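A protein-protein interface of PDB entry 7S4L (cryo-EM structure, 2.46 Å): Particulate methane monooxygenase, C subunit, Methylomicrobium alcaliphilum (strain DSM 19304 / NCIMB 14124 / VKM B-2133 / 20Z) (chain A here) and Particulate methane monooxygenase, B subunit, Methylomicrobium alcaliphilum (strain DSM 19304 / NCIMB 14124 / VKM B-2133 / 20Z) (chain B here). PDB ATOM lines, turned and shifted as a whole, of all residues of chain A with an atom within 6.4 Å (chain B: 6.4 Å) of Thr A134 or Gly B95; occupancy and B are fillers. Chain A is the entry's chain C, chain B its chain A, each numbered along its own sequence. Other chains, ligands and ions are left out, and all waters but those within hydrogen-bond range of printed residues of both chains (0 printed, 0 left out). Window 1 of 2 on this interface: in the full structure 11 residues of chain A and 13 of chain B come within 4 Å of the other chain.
The guanidinium group (NE) of Arg A137 is in hydrogen-bond range of the backbone carbonyl oxygen (O) of Ile A135 (2.4 Å). O of Trp A131 sits at hydrogen-bond distance from OG1 of Thr A134, at 3.2 Å. The backbone carbonyl oxygen of Val B97 sits at hydrogen-bond distance from the backbone NH of Arg B132 (3.0 Å).
Printed residues of chain B within 4 Å of Trp A46: Pro B94 (3.4 Å) and Arg B132 (3.0 Å). Of chain B, only Ile B93 (3.5 Å) and Gly B95 (3.8 Å) come within 4 Å of Thr A134. Of the printed residues of chain B, Ile A135 touches Ile B93 (3.8 Å) and Pro B94 (3.7 Å). Of the printed residues of chain A, Ile B93 touches Thr A134 and Ile A135. Of the printed residues of chain A, Pro B94 touches Trp A46 and Ile A135. Gly B95 touches just one residue of chain A: Thr A134. Printed residues of chain A within 4 Å of Arg B132: Trp A46. The nearest residue of chain A that does not touch Gly B95 is Ile A135 (4.7 Å). The nearest printed residue of chain A that does not touch Ile B93 is Gln A133 (6.4 Å).
O of Ile B93 sits close to O of Thr A134.
Printed residues of chain A that touch a printed residue of chain B: Trp A46, Thr A134 and Ile A135. Hydrophobic or aromatic side chains of chain A within 4 Å of the printed part of chain B: Trp A46 and Ile A135. Of the 9 printed residues of chain B, 4 touch a printed residue of chain A. Hydrophobic or aromatic side chains of chain B within 4 Å of the printed part of chain A: Pro B94. Among the printed residues, 6 pairs touch across the chains.
O of Pro B94 touches CH2 of Trp A46, at 3.4 Å. Trp A46 touches Arg B132. Gly B95 touches Thr A134 (N to CB, 3.8 Å). Ile B93 touches Ile A135. Ile A135 touches Pro B94.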
ATOM      1  N   TRP A  46      29.615 -21.696  -8.522  1.00  0.00           N
ATOM      2  CA  TRP A  46      28.988 -20.719  -9.398  1.00  0.00           C
ATOM      3  C   TRP A  46      29.628 -20.748 -10.776  1.00  0.00           C
ATOM      4  O   TRP A  46      28.973 -21.062 -11.772  1.00  0.00           O
ATOM      5  CB  TRP A  46      29.075 -19.320  -8.796  1.00  0.00           C
ATOM      6  CG  TRP A  46      27.777 -18.621  -8.898  1.00  0.00           C
ATOM      7  CD1 TRP A  46      27.092 -18.016  -7.895  1.00  0.00           C
ATOM      8  CD2 TRP A  46      26.971 -18.494 -10.071  1.00  0.00           C
ATOM      9  NE1 TRP A  46      25.915 -17.499  -8.372  1.00  0.00           N
ATOM     10  CE2 TRP A  46      25.818 -17.782  -9.709  1.00  0.00           C
ATOM     11  CE3 TRP A  46      27.119 -18.902 -11.396  1.00  0.00           C
ATOM     12  CZ2 TRP A  46      24.820 -17.472 -10.621  1.00  0.00           C
ATOM     13  CZ3 TRP A  46      26.132 -18.596 -12.297  1.00  0.00           C
ATOM     14  CH2 TRP A  46      24.995 -17.886 -11.907  1.00  0.00           C
ATOM     15  N   GLY A 129      15.634 -27.019  -8.768  1.00  0.00           N
ATOM     16  CA  GLY A 129      14.679 -26.466  -9.717  1.00  0.00           C
ATOM     17  C   GLY A 129      15.109 -25.112 -10.240  1.00  0.00           C
ATOM     18  O   GLY A 129      15.048 -24.845 -11.438  1.00  0.00           O
ATOM     19  N   THR A 130      15.541 -24.232  -9.338  1.00  0.00           N
ATOM     20  CA  THR A 130      16.087 -22.944  -9.755  1.00  0.00           C
ATOM     21  C   THR A 130      17.251 -23.124 -10.709  1.00  0.00           C
ATOM     22  O   THR A 130      17.330 -22.459 -11.746  1.00  0.00           O
ATOM     23  CB  THR A 130      16.557 -22.150  -8.542  1.00  0.00           C
ATOM     24  OG1 THR A 130      15.448 -21.874  -7.685  1.00  0.00           O
ATOM     25  CG2 THR A 130      17.190 -20.853  -8.984  1.00  0.00           C
ATOM     26  N   TRP A 131      18.167 -24.061 -10.434  1.00  0.00           N
ATOM     27  CA  TRP A 131      19.412 -24.176 -11.258  1.00  0.00           C
ATOM     28  C   TRP A 131      19.187 -24.458 -12.754  1.00  0.00           C
ATOM     29  O   TRP A 131      19.972 -23.928 -13.563  1.00  0.00           O
ATOM     30  CB  TRP A 131      20.401 -25.164 -10.624  1.00  0.00           C
ATOM     31  CG  TRP A 131      21.845 -24.927 -10.958  1.00  0.00           C
ATOM     32  CD1 TRP A 131      22.752 -25.886 -11.296  1.00  0.00           C
ATOM     33  CD2 TRP A 131      22.567 -23.678 -10.973  1.00  0.00           C
ATOM     34  NE1 TRP A 131      23.982 -25.333 -11.517  1.00  0.00           N
ATOM     35  CE2 TRP A 131      23.899 -23.978 -11.334  1.00  0.00           C
ATOM     36  CE3 TRP A 131      22.235 -22.340 -10.723  1.00  0.00           C
ATOM     37  CZ2 TRP A 131      24.884 -23.000 -11.452  1.00  0.00           C
ATOM     38  CZ3 TRP A 131      23.208 -21.373 -10.839  1.00  0.00           C
ATOM     39  CH2 TRP A 131      24.514 -21.700 -11.197  1.00  0.00           C
ATOM     40  N   HIS A 132      18.202 -25.283 -13.116  1.00  0.00           N
ATOM     41  CA  HIS A 132      17.979 -25.665 -14.543  1.00  0.00           C
ATOM     42  C   HIS A 132      17.458 -24.454 -15.275  1.00  0.00           C
ATOM     43  O   HIS A 132      17.959 -24.148 -16.380  1.00  0.00           O
ATOM     44  CB  HIS A 132      16.825 -26.666 -14.664  1.00  0.00           C
ATOM     45  CG  HIS A 132      17.129 -27.824 -13.805  1.00  0.00           C
ATOM     46  ND1 HIS A 132      18.424 -28.065 -13.527  1.00  0.00           N
ATOM     47  CD2 HIS A 132      16.390 -28.742 -13.137  1.00  0.00           C
ATOM     48  CE1 HIS A 132      18.480 -29.058 -12.718  1.00  0.00           C
ATOM     49  NE2 HIS A 132      17.281 -29.545 -12.465  1.00  0.00           N
ATOM     50  N   GLN A 133      16.440 -23.853 -14.667  1.00  0.00           N
ATOM     51  CA  GLN A 133      15.823 -22.679 -15.304  1.00  0.00           C
ATOM     52  C   GLN A 133      16.908 -21.666 -15.641  1.00  0.00           C
ATOM     53  O   GLN A 133      16.642 -20.833 -16.526  1.00  0.00           O
ATOM     54  CB  GLN A 133      14.739 -22.086 -14.405  1.00  0.00           C
ATOM     55  CG  GLN A 133      13.792 -23.122 -13.813  1.00  0.00           C
ATOM     56  CD  GLN A 133      12.901 -23.802 -14.825  1.00  0.00           C
ATOM     57  OE1 GLN A 133      13.231 -24.854 -15.368  1.00  0.00           O
ATOM     58  NE2 GLN A 133      11.744 -23.211 -15.072  1.00  0.00           N
ATOM     59  N   THR A 134      18.100 -21.747 -15.002  1.00  0.00           N
ATOM     60  CA  THR A 134      18.988 -20.663 -15.412  1.00  0.00           C
ATOM     61  C   THR A 134      19.816 -21.062 -16.624  1.00  0.00           C
ATOM     62  O   THR A 134      19.616 -20.546 -17.727  1.00  0.00           O
ATOM     63  CB  THR A 134      19.914 -20.278 -14.259  1.00  0.00           C
ATOM     64  OG1 THR A 134      21.110 -21.058 -14.349  1.00  0.00           O
ATOM     65  CG2 THR A 134      19.246 -20.563 -12.938  1.00  0.00           C
ATOM     66  N   ILE A 135      20.744 -21.991 -16.433  1.00  0.00           N
ATOM     67  CA  ILE A 135      21.622 -22.403 -17.517  1.00  0.00           C
ATOM     68  C   ILE A 135      21.628 -23.914 -17.643  1.00  0.00           C
ATOM     69  O   ILE A 135      21.351 -24.473 -18.708  1.00  0.00           O
ATOM     70  CB  ILE A 135      23.050 -21.880 -17.296  1.00  0.00           C
ATOM     71  CG1 ILE A 135      24.027 -22.561 -18.259  1.00  0.00           C
ATOM     72  CG2 ILE A 135      23.476 -22.115 -15.856  1.00  0.00           C
ATOM     73  CD1 ILE A 135      23.911 -22.099 -19.694  1.00  0.00           C
ATOM     74  N   VAL A 136      21.943 -24.584 -16.543  1.00  0.00           N
ATOM     75  CA  VAL A 136      22.482 -25.934 -16.619  1.00  0.00           C
ATOM     76  C   VAL A 136      21.405 -26.880 -17.135  1.00  0.00           C
ATOM     77  O   VAL A 136      20.477 -27.242 -16.408  1.00  0.00           O
ATOM     78  CB  VAL A 136      23.022 -26.389 -15.265  1.00  0.00           C
ATOM     79  CG1 VAL A 136      23.567 -27.803 -15.368  1.00  0.00           C
ATOM     80  CG2 VAL A 136      24.096 -25.430 -14.817  1.00  0.00           C
ATOM     81  N   ARG A 137      21.538 -27.290 -18.393  1.00  0.00           N
ATOM     82  CA  ARG A 137      20.787 -28.426 -18.896  1.00  0.00           C
ATOM     83  C   ARG A 137      21.332 -29.698 -18.266  1.00  0.00           C
ATOM     84  O   ARG A 137      22.545 -29.912 -18.206  1.00  0.00           O
ATOM     85  CB  ARG A 137      20.881 -28.509 -20.416  1.00  0.00           C
ATOM     86  CG  ARG A 137      19.668 -27.975 -21.148  1.00  0.00           C
ATOM     87  CD  ARG A 137      19.738 -26.472 -21.326  1.00  0.00           C
ATOM     88  NE  ARG A 137      20.872 -25.881 -20.632  1.00  0.00           N
ATOM     89  CZ  ARG A 137      22.015 -25.567 -21.223  1.00  0.00           C
ATOM     90  NH1 ARG A 137      22.173 -25.798 -22.515  1.00  0.00           N
ATOM     91  NH2 ARG A 137      23.002 -25.032 -20.524  1.00  0.00           N
ATOM     92  N   ILE B  91      19.008 -17.089 -25.575  1.00  0.00           N
ATOM     93  CA  ILE B  91      20.371 -16.699 -25.247  1.00  0.00           C
ATOM     94  C   ILE B  91      20.872 -17.612 -24.142  1.00  0.00           C
ATOM     95  O   ILE B  91      20.175 -17.828 -23.145  1.00  0.00           O
ATOM     96  CB  ILE B  91      20.450 -15.228 -24.815  1.00  0.00           C
ATOM     97  CG1 ILE B  91      20.342 -14.326 -26.031  1.00  0.00           C
ATOM     98  CG2 ILE B  91      21.753 -14.964 -24.120  1.00  0.00           C
ATOM     99  CD1 ILE B  91      21.480 -14.502 -26.984  1.00  0.00           C
ATOM    100  N   ILE B  93      23.048 -18.100 -21.121  1.00  0.00           N
ATOM    101  CA  ILE B  93      23.834 -17.459 -20.068  1.00  0.00           C
ATOM    102  C   ILE B  93      23.370 -17.973 -18.721  1.00  0.00           C
ATOM    103  O   ILE B  93      22.229 -18.442 -18.571  1.00  0.00           O
ATOM    104  CB  ILE B  93      23.721 -15.927 -20.112  1.00  0.00           C
ATOM    105  CG1 ILE B  93      22.259 -15.513 -20.221  1.00  0.00           C
ATOM    106  CG2 ILE B  93      24.498 -15.372 -21.274  1.00  0.00           C
ATOM    107  CD1 ILE B  93      22.075 -14.054 -20.483  1.00  0.00           C
ATOM    108  N   PRO B  94      24.222 -17.900 -17.715  1.00  0.00           N
ATOM    109  CA  PRO B  94      23.877 -18.417 -16.379  1.00  0.00           C
ATOM    110  C   PRO B  94      22.951 -17.480 -15.617  1.00  0.00           C
ATOM    111  O   PRO B  94      23.331 -16.790 -14.671  1.00  0.00           O
ATOM    112  CB  PRO B  94      25.252 -18.548 -15.721  1.00  0.00           C
ATOM    113  CG  PRO B  94      26.033 -17.453 -16.327  1.00  0.00           C
ATOM    114  CD  PRO B  94      25.584 -17.345 -17.752  1.00  0.00           C
ATOM    115  N   GLY B  95      21.690 -17.450 -16.023  1.00  0.00           N
ATOM    116  CA  GLY B  95      20.735 -16.553 -15.427  1.00  0.00           C
ATOM    117  C   GLY B  95      20.831 -15.174 -16.032  1.00  0.00           C
ATOM    118  O   GLY B  95      21.703 -14.891 -16.854  1.00  0.00           O
ATOM    119  N   PRO B  96      19.945 -14.288 -15.639  1.00  0.00           N
ATOM    120  CA  PRO B  96      19.927 -12.955 -16.248  1.00  0.00           C
ATOM    121  C   PRO B  96      21.106 -12.093 -15.831  1.00  0.00           C
ATOM    122  O   PRO B  96      20.958 -11.136 -15.068  1.00  0.00           O
ATOM    123  CB  PRO B  96      18.596 -12.382 -15.754  1.00  0.00           C
ATOM    124  CG  PRO B  96      18.353 -13.069 -14.486  1.00  0.00           C
ATOM    125  CD  PRO B  96      18.865 -14.458 -14.659  1.00  0.00           C
ATOM    126  N   VAL B  97      22.295 -12.427 -16.327  1.00  0.00           N
ATOM    127  CA  VAL B  97      23.417 -11.512 -16.178  1.00  0.00           C
ATOM    128  C   VAL B  97      23.294 -10.370 -17.169  1.00  0.00           C
ATOM    129  O   VAL B  97      23.678  -9.235 -16.870  1.00  0.00           O
ATOM    130  CB  VAL B  97      24.746 -12.262 -16.340  1.00  0.00           C
ATOM    131  CG1 VAL B  97      24.824 -13.388 -15.346  1.00  0.00           C
ATOM    132  CG2 VAL B  97      24.872 -12.795 -17.738  1.00  0.00           C
ATOM    133  N   PHE B  98      22.771 -10.649 -18.356  1.00  0.00           N
ATOM    134  CA  PHE B  98      22.258  -9.645 -19.268  1.00  0.00           C
ATOM    135  C   PHE B  98      20.741  -9.711 -19.254  1.00  0.00           C
ATOM    136  O   PHE B  98      20.150 -10.642 -18.708  1.00  0.00           O
ATOM    137  CB  PHE B  98      22.750  -9.875 -20.697  1.00  0.00           C
ATOM    138  CG  PHE B  98      24.229  -9.776 -20.860  1.00  0.00           C
ATOM    139  CD1 PHE B  98      25.025 -10.887 -20.707  1.00  0.00           C
ATOM    140  CD2 PHE B  98      24.819  -8.578 -21.193  1.00  0.00           C
ATOM    141  CE1 PHE B  98      26.379 -10.798 -20.868  1.00  0.00           C
ATOM    142  CE2 PHE B  98      26.172  -8.488 -21.357  1.00  0.00           C
ATOM    143  CZ  PHE B  98      26.952  -9.598 -21.193  1.00  0.00           C
ATOM    144  N   ARG B 131      23.935  -6.496 -16.908  1.00  0.00           N
ATOM    145  CA  ARG B 131      23.231  -6.361 -15.642  1.00  0.00           C
ATOM    146  C   ARG B 131      24.060  -6.739 -14.428  1.00  0.00           C
ATOM    147  O   ARG B 131      23.954  -6.081 -13.395  1.00  0.00           O
ATOM    148  CB  ARG B 131      21.962  -7.213 -15.660  1.00  0.00           C
ATOM    149  CG  ARG B 131      21.200  -7.211 -14.359  1.00  0.00           C
ATOM    150  CD  ARG B 131      19.828  -7.802 -14.546  1.00  0.00           C
ATOM    151  NE  ARG B 131      19.084  -7.852 -13.298  1.00  0.00           N
ATOM    152  CZ  ARG B 131      18.875  -8.962 -12.605  1.00  0.00           C
ATOM    153  NH1 ARG B 131      19.353 -10.112 -13.044  1.00  0.00           N
ATOM    154  NH2 ARG B 131      18.187  -8.923 -11.479  1.00  0.00           N
ATOM    155  N   ARG B 132      24.881  -7.781 -14.515  1.00  0.00           N
ATOM    156  CA  ARG B 132      25.592  -8.293 -13.354  1.00  0.00           C
ATOM    157  C   ARG B 132      27.075  -8.447 -13.663  1.00  0.00           C
ATOM    158  O   ARG B 132      27.436  -9.112 -14.647  1.00  0.00           O
ATOM    159  CB  ARG B 132      25.006  -9.630 -12.916  1.00  0.00           C
ATOM    160  CG  ARG B 132      25.670 -10.193 -11.695  1.00  0.00           C
ATOM    161  CD  ARG B 132      24.674 -10.904 -10.823  1.00  0.00           C
ATOM    162  NE  ARG B 132      24.492 -12.289 -11.230  1.00  0.00           N
ATOM    163  CZ  ARG B 132      25.218 -13.298 -10.764  1.00  0.00           C
ATOM    164  NH1 ARG B 132      24.986 -14.529 -11.184  1.00  0.00           N
ATOM    165  NH2 ARG B 132      26.176 -13.070  -9.881  1.00  0.00           N
